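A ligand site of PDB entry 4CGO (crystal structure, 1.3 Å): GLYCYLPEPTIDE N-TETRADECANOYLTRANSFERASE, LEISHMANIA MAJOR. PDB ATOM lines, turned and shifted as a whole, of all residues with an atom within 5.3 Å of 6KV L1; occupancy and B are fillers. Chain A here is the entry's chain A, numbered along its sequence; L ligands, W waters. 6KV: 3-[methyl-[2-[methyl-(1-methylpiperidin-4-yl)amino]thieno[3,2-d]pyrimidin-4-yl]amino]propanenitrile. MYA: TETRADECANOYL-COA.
Merely in contact with 6KV L1: Asn 157 (3.1 Å), Phe 80 (3.3 Å), Thr 193 (3.4 Å), His 209 (3.6 Å), Tyr 82 (3.7 Å), His 388 (3.7 Å), Ile 318 (3.8 Å), Met 410 (3.8 Å), Gly 387 (3.9 Å) and Val 71 (3.99 Å).
Hydrophobic or aromatic side chains that line 6KV L1: Val 71, Phe 80, Tyr 207, His 209, Ile 318 and Tyr 335.
Within 4 Å of 6KV L1: Val 71, Phe 80, Tyr 82, Asn 157, Thr 193, Gly 195, Tyr 207, His 209, Ile 318, Tyr 335, Gly 387, His 388, Met 410 and Leu 411.
Along chain A the residues within 4 Å of 6KV L1 span positions 71 to 411.
The nearest printed residue that does not touch 6KV L1 is Ala 194 (4.05 Å).
OH of Tyr 335 lies within hydrogen-bond range of N3 of 6KV L1.
The chain-end carboxylate (O) of Leu 411 lies within salt-bridge range of a nitrogen (N5) of 6KV L1, 3.2 Å away.
The side-chain hydroxyl (OH) of Tyr 207 sits at hydrogen-bond distance from a nitrogen (N2) of 6KV L1, at 3.2 Å.
N of Gly 195 sits at hydrogen-bond distance from N1 of 6KV L1.
A nitrogen (N1) of 6KV L2 sits at hydrogen-bond distance from the side-chain amide nitrogen (ND2) of Asn 366, at 3.2 Å.
The side-chain amide nitrogen (ND2) of Asn 157 sits at hydrogen-bond distance from the chain-end carboxylate (O) of Leu 411, 2.8 Å away.
OD1 of Asn 157 lies within hydrogen-bond range of OH of Tyr 70 (3.4 Å).
The chain-end carboxylate (OXT) of Leu 411 lies within hydrogen-bond range of the side-chain hydroxyl (OH) of Tyr 82 (2.6 Å).
N of Tyr 207 lies within hydrogen-bond range of O of Gly 387.
The backbone carbonyl oxygen (O) of Val 71 sits at hydrogen-bond distance from the backbone NH (N) of Phe 80, at 3.0 Å.
ND1 of His 209 sits at hydrogen-bond distance from OD1 of Asn 366, 2.7 Å away.
Water W4 lies within hydrogen-bond range of the side-chain hydroxyl (OH) of Tyr 70 (2.6 Å), the side-chain amide oxygen (OD1) of Asn 157 (2.7 Å), the side-chain hydroxyl (OH) of Tyr 82 (2.8 Å) and the chain-end carboxylate (O) of Leu 411 (3.1 Å).
Water W1 lies within hydrogen-bond range of the backbone NH of Val 196 (2.9 Å), a nitrogen (N1) of 6KV L1 (3.0 Å) and the backbone NH of Gly 195 (3.0 Å).
Water W2 lies within hydrogen-bond range of N3 of 6KV L2 (3.1 Å), S of 6KV L1 (3.4 Å) and N of Gly 387 (3.5 Å).
Water W5 lies within hydrogen-bond range of O of Met 410 (2.7 Å) and OXT of Leu 411 (2.8 Å).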
ATOM      1  N   TYR A  70     -16.814  -9.552  -9.461  1.00  0.00           N
ATOM      2  CA  TYR A  70     -16.882 -10.993  -9.148  1.00  0.00           C
ATOM      3  C   TYR A  70     -17.409 -11.238  -7.749  1.00  0.00           C
ATOM      4  O   TYR A  70     -17.999 -10.370  -7.120  1.00  0.00           O
ATOM      5  CB  TYR A  70     -15.538 -11.664  -9.433  1.00  0.00           C
ATOM      6  CG  TYR A  70     -15.642 -13.206  -9.646  1.00  0.00           C
ATOM      7  CD1 TYR A  70     -16.546 -13.780 -10.513  1.00  0.00           C
ATOM      8  CD2 TYR A  70     -14.688 -14.024  -9.048  1.00  0.00           C
ATOM      9  CE1 TYR A  70     -16.569 -15.155 -10.746  1.00  0.00           C
ATOM     10  CE2 TYR A  70     -14.711 -15.439  -9.261  1.00  0.00           C
ATOM     11  CZ  TYR A  70     -15.656 -15.941 -10.114  1.00  0.00           C
ATOM     12  OH  TYR A  70     -15.659 -17.302 -10.293  1.00  0.00           O
ATOM     13  N   VAL A  71     -17.270 -12.475  -7.226  1.00  0.00           N
ATOM     14  CA  VAL A  71     -18.069 -12.844  -6.057  1.00  0.00           C
ATOM     15  C   VAL A  71     -17.663 -12.037  -4.813  1.00  0.00           C
ATOM     16  O   VAL A  71     -16.449 -11.777  -4.561  1.00  0.00           O
ATOM     17  CB  VAL A  71     -17.838 -14.327  -5.686  1.00  0.00           C
ATOM     18  CG1 VAL A  71     -18.819 -14.710  -4.603  1.00  0.00           C
ATOM     19  CG2 VAL A  71     -17.956 -15.290  -6.864  1.00  0.00           C
ATOM     20  N   PHE A  80     -13.522 -11.096  -4.257  1.00  0.00           N
ATOM     21  CA  PHE A  80     -12.254 -11.685  -4.809  1.00  0.00           C
ATOM     22  C   PHE A  80     -11.528 -10.762  -5.749  1.00  0.00           C
ATOM     23  O   PHE A  80     -12.137 -10.032  -6.535  1.00  0.00           O
ATOM     24  CB  PHE A  80     -12.580 -12.971  -5.573  1.00  0.00           C
ATOM     25  CG  PHE A  80     -13.045 -14.073  -4.678  1.00  0.00           C
ATOM     26  CD1 PHE A  80     -12.223 -14.567  -3.683  1.00  0.00           C
ATOM     27  CD2 PHE A  80     -14.347 -14.591  -4.841  1.00  0.00           C
ATOM     28  CE1 PHE A  80     -12.690 -15.612  -2.834  1.00  0.00           C
ATOM     29  CE2 PHE A  80     -14.791 -15.647  -4.012  1.00  0.00           C
ATOM     30  CZ  PHE A  80     -14.005 -16.109  -2.997  1.00  0.00           C
ATOM     31  N   TYR A  82      -8.690 -12.004  -7.862  1.00  0.00           N
ATOM     32  CA  TYR A  82      -7.772 -12.915  -8.528  1.00  0.00           C
ATOM     33  C   TYR A  82      -6.777 -12.117  -9.375  1.00  0.00           C
ATOM     34  O   TYR A  82      -7.180 -11.200 -10.121  1.00  0.00           O
ATOM     35  CB  TYR A  82      -8.569 -13.811  -9.501  1.00  0.00           C
ATOM     36  CG  TYR A  82      -9.377 -14.925  -8.888  1.00  0.00           C
ATOM     37  CD1 TYR A  82     -10.669 -14.735  -8.421  1.00  0.00           C
ATOM     38  CD2 TYR A  82      -8.821 -16.230  -8.795  1.00  0.00           C
ATOM     39  CE1 TYR A  82     -11.379 -15.805  -7.863  1.00  0.00           C
ATOM     40  CE2 TYR A  82      -9.560 -17.285  -8.290  1.00  0.00           C
ATOM     41  CZ  TYR A  82     -10.834 -17.065  -7.850  1.00  0.00           C
ATOM     42  OH  TYR A  82     -11.631 -18.125  -7.385  1.00  0.00           O
ATOM     43  N   ASN A 157     -15.646 -21.776 -15.088  1.00  0.00           N
ATOM     44  CA  ASN A 157     -15.286 -20.922 -13.946  1.00  0.00           C
ATOM     45  C   ASN A 157     -15.376 -19.480 -14.391  1.00  0.00           C
ATOM     46  O   ASN A 157     -15.484 -19.178 -15.611  1.00  0.00           O
ATOM     47  CB  ASN A 157     -13.827 -21.295 -13.474  1.00  0.00           C
ATOM     48  CG  ASN A 157     -13.558 -21.011 -12.011  1.00  0.00           C
ATOM     49  OD1 ASN A 157     -14.201 -20.208 -11.369  1.00  0.00           O
ATOM     50  ND2 ASN A 157     -12.566 -21.726 -11.453  1.00  0.00           N
ATOM     51  N   THR A 193     -18.431 -25.500 -10.132  1.00  0.00           N
ATOM     52  CA  THR A 193     -18.760 -25.294  -8.676  1.00  0.00           C
ATOM     53  C   THR A 193     -19.332 -23.980  -8.489  1.00  0.00           C
ATOM     54  O   THR A 193     -19.083 -23.014  -9.263  1.00  0.00           O
ATOM     55  CB  THR A 193     -17.583 -25.519  -7.761  1.00  0.00           C
ATOM     56  OG1 THR A 193     -16.508 -24.571  -8.100  1.00  0.00           O
ATOM     57  CG2 THR A 193     -17.037 -26.965  -7.845  1.00  0.00           C
ATOM     58  N   ALA A 194     -20.159 -23.812  -7.435  1.00  0.00           N
ATOM     59  CA  ALA A 194     -20.648 -22.484  -7.004  1.00  0.00           C
ATOM     60  C   ALA A 194     -21.029 -22.581  -5.540  1.00  0.00           C
ATOM     61  O   ALA A 194     -21.241 -23.660  -5.010  1.00  0.00           O
ATOM     62  CB  ALA A 194     -21.894 -22.107  -7.794  1.00  0.00           C
ATOM     63  N   GLY A 195     -21.116 -21.410  -4.900  1.00  0.00           N
ATOM     64  CA  GLY A 195     -21.656 -21.306  -3.542  1.00  0.00           C
ATOM     65  C   GLY A 195     -23.163 -21.438  -3.540  1.00  0.00           C
ATOM     66  O   GLY A 195     -23.772 -22.052  -2.604  1.00  0.00           O
ATOM     67  N   VAL A 196     -23.796 -20.887  -4.513  1.00  0.00           N
ATOM     68  CA  VAL A 196     -25.283 -20.865  -4.573  1.00  0.00           C
ATOM     69  C   VAL A 196     -25.780 -22.267  -4.872  1.00  0.00           C
ATOM     70  O   VAL A 196     -25.118 -23.102  -5.542  1.00  0.00           O
ATOM     71  CB  VAL A 196     -25.801 -19.822  -5.507  1.00  0.00           C
ATOM     72  CG1 VAL A 196     -25.448 -18.467  -4.901  1.00  0.00           C
ATOM     73  CG2 VAL A 196     -25.354 -20.018  -6.958  1.00  0.00           C
ATOM     74  N   TYR A 207     -16.819 -24.971   3.610  1.00  0.00           N
ATOM     75  CA  TYR A 207     -15.501 -24.321   3.705  1.00  0.00           C
ATOM     76  C   TYR A 207     -14.971 -24.355   5.099  1.00  0.00           C
ATOM     77  O   TYR A 207     -15.754 -24.290   6.105  1.00  0.00           O
ATOM     78  CB  TYR A 207     -15.605 -22.863   3.291  1.00  0.00           C
ATOM     79  CG  TYR A 207     -15.342 -22.672   1.781  1.00  0.00           C
ATOM     80  CD1 TYR A 207     -14.045 -22.579   1.310  1.00  0.00           C
ATOM     81  CD2 TYR A 207     -16.402 -22.654   0.885  1.00  0.00           C
ATOM     82  CE1 TYR A 207     -13.821 -22.491  -0.083  1.00  0.00           C
ATOM     83  CE2 TYR A 207     -16.138 -22.555  -0.515  1.00  0.00           C
ATOM     84  CZ  TYR A 207     -14.882 -22.503  -0.945  1.00  0.00           C
ATOM     85  OH  TYR A 207     -14.639 -22.524  -2.326  1.00  0.00           O
ATOM     86  N   HIS A 209     -11.497 -22.691   7.475  1.00  0.00           N
ATOM     87  CA  HIS A 209     -10.515 -21.594   7.507  1.00  0.00           C
ATOM     88  C   HIS A 209      -9.571 -21.847   8.671  1.00  0.00           C
ATOM     89  O   HIS A 209      -9.989 -22.280   9.727  1.00  0.00           O
ATOM     90  CB  HIS A 209     -11.246 -20.245   7.651  1.00  0.00           C
ATOM     91  CG  HIS A 209     -12.449 -20.126   6.751  1.00  0.00           C
ATOM     92  ND1 HIS A 209     -12.307 -19.969   5.392  1.00  0.00           N
ATOM     93  CD2 HIS A 209     -13.793 -20.302   6.976  1.00  0.00           C
ATOM     94  CE1 HIS A 209     -13.507 -20.004   4.821  1.00  0.00           C
ATOM     95  NE2 HIS A 209     -14.420 -20.233   5.730  1.00  0.00           N
ATOM     96  N   ILE A 318      -5.308 -16.515  -3.538  1.00  0.00           N
ATOM     97  CA  ILE A 318      -6.387 -15.632  -4.059  1.00  0.00           C
ATOM     98  C   ILE A 318      -6.550 -14.495  -3.083  1.00  0.00           C
ATOM     99  O   ILE A 318      -7.053 -14.748  -1.998  1.00  0.00           O
ATOM    100  CB  ILE A 318      -7.739 -16.355  -4.300  1.00  0.00           C
ATOM    101  CG1 ILE A 318      -7.548 -17.685  -5.087  1.00  0.00           C
ATOM    102  CG2 ILE A 318      -8.744 -15.366  -4.947  1.00  0.00           C
ATOM    103  CD1 ILE A 318      -8.845 -18.516  -5.108  1.00  0.00           C
ATOM    104  N   TYR A 335      -4.955 -21.169  -0.332  1.00  0.00           N
ATOM    105  CA  TYR A 335      -5.953 -22.249  -0.474  1.00  0.00           C
ATOM    106  C   TYR A 335      -5.224 -23.547  -0.632  1.00  0.00           C
ATOM    107  O   TYR A 335      -4.267 -23.694  -1.452  1.00  0.00           O
ATOM    108  CB  TYR A 335      -6.784 -22.046  -1.762  1.00  0.00           C
ATOM    109  CG  TYR A 335      -7.864 -21.010  -1.576  1.00  0.00           C
ATOM    110  CD1 TYR A 335      -7.555 -19.673  -1.532  1.00  0.00           C
ATOM    111  CD2 TYR A 335      -9.193 -21.381  -1.519  1.00  0.00           C
ATOM    112  CE1 TYR A 335      -8.559 -18.705  -1.368  1.00  0.00           C
ATOM    113  CE2 TYR A 335     -10.211 -20.417  -1.353  1.00  0.00           C
ATOM    114  CZ  TYR A 335      -9.830 -19.116  -1.296  1.00  0.00           C
ATOM    115  OH  TYR A 335     -10.847 -18.093  -1.198  1.00  0.00           O
ATOM    116  N   ASN A 366      -7.532 -21.423   3.502  1.00  0.00           N
ATOM    117  CA  ASN A 366      -8.906 -21.911   3.227  1.00  0.00           C
ATOM    118  C   ASN A 366      -8.880 -23.262   2.532  1.00  0.00           C
ATOM    119  O   ASN A 366      -7.925 -23.581   1.752  1.00  0.00           O
ATOM    120  CB  ASN A 366      -9.575 -20.910   2.254  1.00  0.00           C
ATOM    121  CG  ASN A 366      -9.816 -19.561   2.909  1.00  0.00           C
ATOM    122  OD1 ASN A 366     -10.060 -19.416   4.059  1.00  0.00           O
ATOM    123  ND2 ASN A 366      -9.603 -18.476   2.130  1.00  0.00           N
ATOM    124  N   GLY A 387     -19.757 -20.898   4.588  1.00  0.00           N
ATOM    125  CA  GLY A 387     -19.946 -21.124   3.123  1.00  0.00           C
ATOM    126  C   GLY A 387     -19.916 -22.592   2.822  1.00  0.00           C
ATOM    127  O   GLY A 387     -19.369 -23.433   3.577  1.00  0.00           O
ATOM    128  N   HIS A 388     -20.195 -22.807   1.549  1.00  0.00           N
ATOM    129  CA  HIS A 388     -20.070 -24.108   1.041  1.00  0.00           C
ATOM    130  C   HIS A 388     -19.667 -23.936  -0.383  1.00  0.00           C
ATOM    131  O   HIS A 388     -19.883 -22.968  -1.075  1.00  0.00           O
ATOM    132  CB  HIS A 388     -21.471 -24.739   0.931  1.00  0.00           C
ATOM    133  CG  HIS A 388     -22.157 -24.978   2.244  1.00  0.00           C
ATOM    134  ND1 HIS A 388     -22.921 -24.039   2.889  1.00  0.00           N
ATOM    135  CD2 HIS A 388     -22.164 -26.083   3.015  1.00  0.00           C
ATOM    136  CE1 HIS A 388     -23.407 -24.570   3.995  1.00  0.00           C
ATOM    137  NE2 HIS A 388     -22.952 -25.800   4.098  1.00  0.00           N
ATOM    138  N   LEU A 389     -19.286 -25.062  -0.836  1.00  0.00           N
ATOM    139  CA  LEU A 389     -18.984 -25.241  -2.275  1.00  0.00           C
ATOM    140  C   LEU A 389     -19.758 -26.409  -2.791  1.00  0.00           C
ATOM    141  O   LEU A 389     -19.565 -27.557  -2.285  1.00  0.00           O
ATOM    142  CB  LEU A 389     -17.515 -25.365  -2.593  1.00  0.00           C
ATOM    143  CG  LEU A 389     -17.143 -25.141  -4.067  1.00  0.00           C
ATOM    144  CD1 LEU A 389     -17.451 -23.697  -4.561  1.00  0.00           C
ATOM    145  CD2 LEU A 389     -15.716 -25.478  -4.381  1.00  0.00           C
ATOM    146  N   MET A 410     -11.280 -26.906  -7.479  1.00  0.00           N
ATOM    147  CA  MET A 410     -11.763 -25.912  -8.384  1.00  0.00           C
ATOM    148  C   MET A 410     -11.206 -24.517  -7.918  1.00  0.00           C
ATOM    149  O   MET A 410     -11.393 -24.173  -6.748  1.00  0.00           O
ATOM    150  CB  MET A 410     -13.281 -26.080  -8.338  1.00  0.00           C
ATOM    151  CG  MET A 410     -13.633 -27.398  -9.094  1.00  0.00           C
ATOM    152  SD  MET A 410     -13.365 -27.331 -10.877  1.00  0.00           S
ATOM    153  CE  MET A 410     -15.001 -26.834 -11.292  1.00  0.00           C
ATOM    154  N   LEU A 411     -10.580 -23.798  -8.834  1.00  0.00           N
ATOM    155  CA  LEU A 411      -9.915 -22.539  -8.454  1.00  0.00           C
ATOM    156  C   LEU A 411     -10.874 -21.383  -8.228  1.00  0.00           C
ATOM    157  O   LEU A 411     -12.045 -21.285  -8.708  1.00  0.00           O
ATOM    158  CB  LEU A 411      -8.908 -22.183  -9.608  1.00  0.00           C
ATOM    159  CG  LEU A 411      -7.865 -23.253  -9.806  1.00  0.00           C
ATOM    160  CD1 LEU A 411      -7.024 -22.739 -11.002  1.00  0.00           C
ATOM    161  CD2 LEU A 411      -6.933 -23.528  -8.613  1.00  0.00           C
ATOM    162  OXT LEU A 411     -10.532 -20.486  -7.340  1.00  0.00           O
HETATM  163  N1  6KV L   1     -19.228 -18.903  -5.755  1.00  0.00           N
HETATM  164  C3  6KV L   1     -18.823 -18.752  -4.777  1.00  0.00           C
HETATM  165  C2  6KV L   1     -18.428 -18.679  -3.377  1.00  0.00           C
HETATM  166  C1  6KV L   1     -18.238 -20.005  -2.527  1.00  0.00           C
HETATM  167  N   6KV L   1     -17.611 -19.551  -1.343  1.00  0.00           N
HETATM  168  C   6KV L   1     -18.583 -19.546  -0.196  1.00  0.00           C
HETATM  169  C4  6KV L   1     -16.218 -19.312  -1.212  1.00  0.00           C
HETATM  170  C9  6KV L   1     -15.479 -18.963  -0.169  1.00  0.00           C
HETATM  171  S   6KV L   1     -16.172 -18.786   1.386  1.00  0.00           S
HETATM  172  C8  6KV L   1     -14.953 -18.341   1.993  1.00  0.00           C
HETATM  173  C7  6KV L   1     -13.619 -18.478   1.206  1.00  0.00           C
HETATM  174  C6  6KV L   1     -14.078 -18.847  -0.115  1.00  0.00           C
HETATM  175  N3  6KV L   1     -13.406 -19.023  -1.391  1.00  0.00           N
HETATM  176  C5  6KV L   1     -14.218 -19.307  -2.403  1.00  0.00           C
HETATM  177  N2  6KV L   1     -15.544 -19.441  -2.353  1.00  0.00           N
HETATM  178  N4  6KV L   1     -13.765 -19.502  -3.681  1.00  0.00           N
HETATM  179  C10 6KV L   1     -12.381 -19.196  -3.972  1.00  0.00           C
HETATM  180  C11 6KV L   1     -14.627 -20.139  -4.810  1.00  0.00           C
HETATM  181  C16 6KV L   1     -14.933 -19.051  -5.873  1.00  0.00           C
HETATM  182  C15 6KV L   1     -15.776 -19.829  -7.088  1.00  0.00           C
HETATM  183  N5  6KV L   1     -15.032 -20.921  -7.594  1.00  0.00           N
HETATM  184  C14 6KV L   1     -15.630 -21.396  -8.902  1.00  0.00           C
HETATM  185  C13 6KV L   1     -14.447 -21.916  -6.705  1.00  0.00           C
HETATM  186  C12 6KV L   1     -13.767 -21.240  -5.482  1.00  0.00           C
HETATM  187  N1  6KV L   2     -10.607 -15.471   1.951  1.00  0.00           N
HETATM  188  C3  6KV L   2     -11.581 -15.224   1.349  1.00  0.00           C
HETATM  189  C2  6KV L   2     -12.811 -15.002   0.644  1.00  0.00           C
HETATM  190  C1  6KV L   2     -13.144 -13.483   0.705  1.00  0.00           C
HETATM  191  N   6KV L   2     -14.533 -13.482   0.131  1.00  0.00           N
HETATM  192  C   6KV L   2     -14.725 -12.984  -1.239  1.00  0.00           C
HETATM  193  C4  6KV L   2     -15.614 -14.027   0.782  1.00  0.00           C
HETATM  194  C9  6KV L   2     -16.883 -14.367   0.235  1.00  0.00           C
HETATM  195  S   6KV L   2     -17.470 -14.349  -1.345  1.00  0.00           S
HETATM  196  C8  6KV L   2     -19.046 -15.001  -0.979  1.00  0.00           C
HETATM  197  C7  6KV L   2     -19.083 -15.264   0.414  1.00  0.00           C
HETATM  198  C6  6KV L   2     -17.841 -14.940   1.083  1.00  0.00           C
HETATM  199  N3  6KV L   2     -17.541 -15.083   2.425  1.00  0.00           N
HETATM  200  C5  6KV L   2     -16.319 -14.765   2.923  1.00  0.00           C
HETATM  201  N2  6KV L   2     -15.375 -14.221   2.080  1.00  0.00           N
HETATM  202  N4  6KV L   2     -15.953 -14.884   4.300  1.00  0.00           N
HETATM  203  C10 6KV L   2     -14.661 -14.398   4.749  1.00  0.00           C
HETATM  204  C11 6KV L   2     -16.952 -15.379   5.261  1.00  0.00           C
HETATM  205  C16 6KV L   2     -17.520 -14.091   5.863  1.00  0.00           C
HETATM  206  C15 6KV L   2     -18.466 -14.425   7.018  1.00  0.00           C
HETATM  207  N5  6KV L   2     -17.686 -15.316   7.912  1.00  0.00           N
HETATM  208  C14 6KV L   2     -17.398 -14.834   9.262  1.00  0.00           C
HETATM  209  C13 6KV L   2     -17.197 -16.644   7.481  1.00  0.00           C
HETATM  210  C12 6KV L   2     -16.274 -16.359   6.283  1.00  0.00           C
HETATM  211  S1  MYA L   3     -19.651 -19.707  -9.872  1.00  0.00           S
HETATM  212  C2  MYA L   3     -19.243 -17.905  -9.707  1.00  0.00           C
HETATM  213  C3  MYA L   3     -20.417 -17.125 -10.259  1.00  0.00           C
HETATM  214  N4  MYA L   3     -20.111 -15.668 -10.282  1.00  0.00           N
HETATM  215  C5  MYA L   3     -20.467 -14.817  -9.363  1.00  0.00           C
HETATM  216  O5  MYA L   3     -21.136 -15.143  -8.367  1.00  0.00           O
HETATM  217  C6  MYA L   3     -20.032 -13.367  -9.608  1.00  0.00           C
HETATM  218  C7  MYA L   3     -21.072 -12.344  -9.078  1.00  0.00           C
HETATM  219  N8  MYA L   3     -22.381 -12.472  -9.750  1.00  0.00           N
HETATM  220  C9  MYA L   3     -22.633 -12.307 -11.043  1.00  0.00           C
HETATM  221  O9  MYA L   3     -21.692 -11.979 -11.795  1.00  0.00           O
HETATM  222  C10 MYA L   3     -24.015 -12.544 -11.503  1.00  0.00           C
HETATM  223  O10 MYA L   3     -24.887 -12.457 -10.367  1.00  0.00           O
HETATM  224  C11 MYA L   3     -24.146 -13.935 -12.224  1.00  0.00           C
HETATM  225  C12 MYA L   3     -25.568 -14.226 -12.573  1.00  0.00           C
HETATM  226  C13 MYA L   3     -23.692 -15.149 -11.386  1.00  0.00           C
HETATM  227  C14 MYA L   3     -23.304 -13.916 -13.524  1.00  0.00           C
HETATM  228  N1A MYA L   3     -24.104 -20.401 -11.840  1.00  0.00           N
HETATM  229  O1A MYA L   3     -30.534 -12.502 -14.823  1.00  0.00           O
HETATM  230  P1A MYA L   3     -29.247 -13.270 -14.821  1.00  0.00           P
HETATM  231  C1X MYA L   3     -28.703 -18.393 -12.709  1.00  0.00           C
HETATM  232  C2A MYA L   3     -25.052 -20.778 -12.716  1.00  0.00           C
HETATM  233  O2A MYA L   3     -28.260 -12.964 -15.822  1.00  0.00           O
HETATM  234  P2A MYA L   3     -27.380 -12.247 -12.861  1.00  0.00           P
HETATM  235  C2M MYA L   3     -19.074 -20.015 -11.495  1.00  0.00           C
HETATM  236  O2M MYA L   3     -18.363 -19.191 -12.082  1.00  0.00           O
HETATM  237  C2X MYA L   3     -29.975 -18.096 -11.895  1.00  0.00           C
HETATM  238  O2X MYA L   3     -30.337 -19.241 -11.129  1.00  0.00           O
HETATM  239  N3A MYA L   3     -26.236 -20.135 -12.854  1.00  0.00           N
HETATM  240  O3A MYA L   3     -28.607 -13.131 -13.311  1.00  0.00           O
HETATM  241  C3M MYA L   3     -19.537 -21.287 -12.118  1.00  0.00           C
HETATM  242  C3X MYA L   3     -30.943 -17.772 -13.038  1.00  0.00           C
HETATM  243  O3X MYA L   3     -31.380 -18.972 -13.689  1.00  0.00           O
HETATM  244  P3X MYA L   3     -32.890 -19.502 -13.298  1.00  0.00           P
HETATM  245  C4A MYA L   3     -26.450 -19.059 -12.027  1.00  0.00           C
HETATM  246  O4A MYA L   3     -27.351 -11.039 -13.548  1.00  0.00           O
HETATM  247  C4M MYA L   3     -20.599 -20.915 -13.199  1.00  0.00           C
HETATM  248  C4X MYA L   3     -30.126 -16.980 -14.025  1.00  0.00           C
HETATM  249  O4X MYA L   3     -28.745 -17.308 -13.669  1.00  0.00           O
HETATM  250  C5A MYA L   3     -25.492 -18.655 -11.134  1.00  0.00           C
HETATM  251  O5A MYA L   3     -27.472 -12.237 -11.405  1.00  0.00           O
HETATM  252  C5M MYA L   3     -21.284 -22.109 -13.813  1.00  0.00           C
HETATM  253  C5X MYA L   3     -30.249 -15.473 -13.894  1.00  0.00           C
HETATM  254  O5X MYA L   3     -29.484 -14.844 -14.856  1.00  0.00           O
HETATM  255  C6A MYA L   3     -24.307 -19.352 -11.036  1.00  0.00           C
HETATM  256  N6A MYA L   3     -23.280 -19.060 -10.156  1.00  0.00           N
HETATM  257  O6A MYA L   3     -26.061 -13.071 -13.344  1.00  0.00           O
HETATM  258  C6M MYA L   3     -22.208 -21.715 -14.967  1.00  0.00           C
HETATM  259  N7A MYA L   3     -26.010 -17.528 -10.470  1.00  0.00           N
HETATM  260  O7A MYA L   3     -33.067 -20.737 -14.063  1.00  0.00           O
HETATM  261  C7M MYA L   3     -22.979 -22.902 -15.588  1.00  0.00           C
HETATM  262  C8A MYA L   3     -27.254 -17.288 -10.958  1.00  0.00           C
HETATM  263  O8A MYA L   3     -33.769 -18.410 -13.682  1.00  0.00           O
HETATM  264  C8M MYA L   3     -22.043 -23.682 -16.530  1.00  0.00           C
HETATM  265  N9A MYA L   3     -27.492 -18.239 -11.903  1.00  0.00           N
HETATM  266  O9A MYA L   3     -32.866 -19.737 -11.804  1.00  0.00           O
HETATM  267  C9M MYA L   3     -22.828 -24.801 -17.288  1.00  0.00           C
HETATM  268  CAM MYA L   3     -21.963 -25.604 -18.252  1.00  0.00           C
HETATM  269  CBM MYA L   3     -21.718 -24.830 -19.559  1.00  0.00           C
HETATM  270  CCM MYA L   3     -20.760 -25.596 -20.525  1.00  0.00           C
HETATM  271  CDM MYA L   3     -21.381 -26.916 -20.981  1.00  0.00           C
HETATM  272  CEM MYA L   3     -20.447 -27.649 -21.983  1.00  0.00           C
HETATM  273  CFM MYA L   3     -20.940 -29.044 -22.335  1.00  0.00           C
HETATM  274  O   HOH W   1     -22.212 -18.770  -5.811  1.00  0.00           O
HETATM  275  O   HOH W   2     -18.696 -17.787   3.430  1.00  0.00           O
HETATM  276  O   HOH W   3     -21.415 -17.588  -3.106  1.00  0.00           O
HETATM  277  O   HOH W   4     -13.785 -18.756  -9.123  1.00  0.00           O
HETATM  278  O   HOH W   5     -10.491 -22.198  -5.088  1.00  0.00           O
HETATM  279  O   HOH W   6     -16.650 -23.364 -11.074  1.00  0.00           O
HETATM  280  O   HOH W   7     -21.719 -18.671  -0.830  1.00  0.00           O
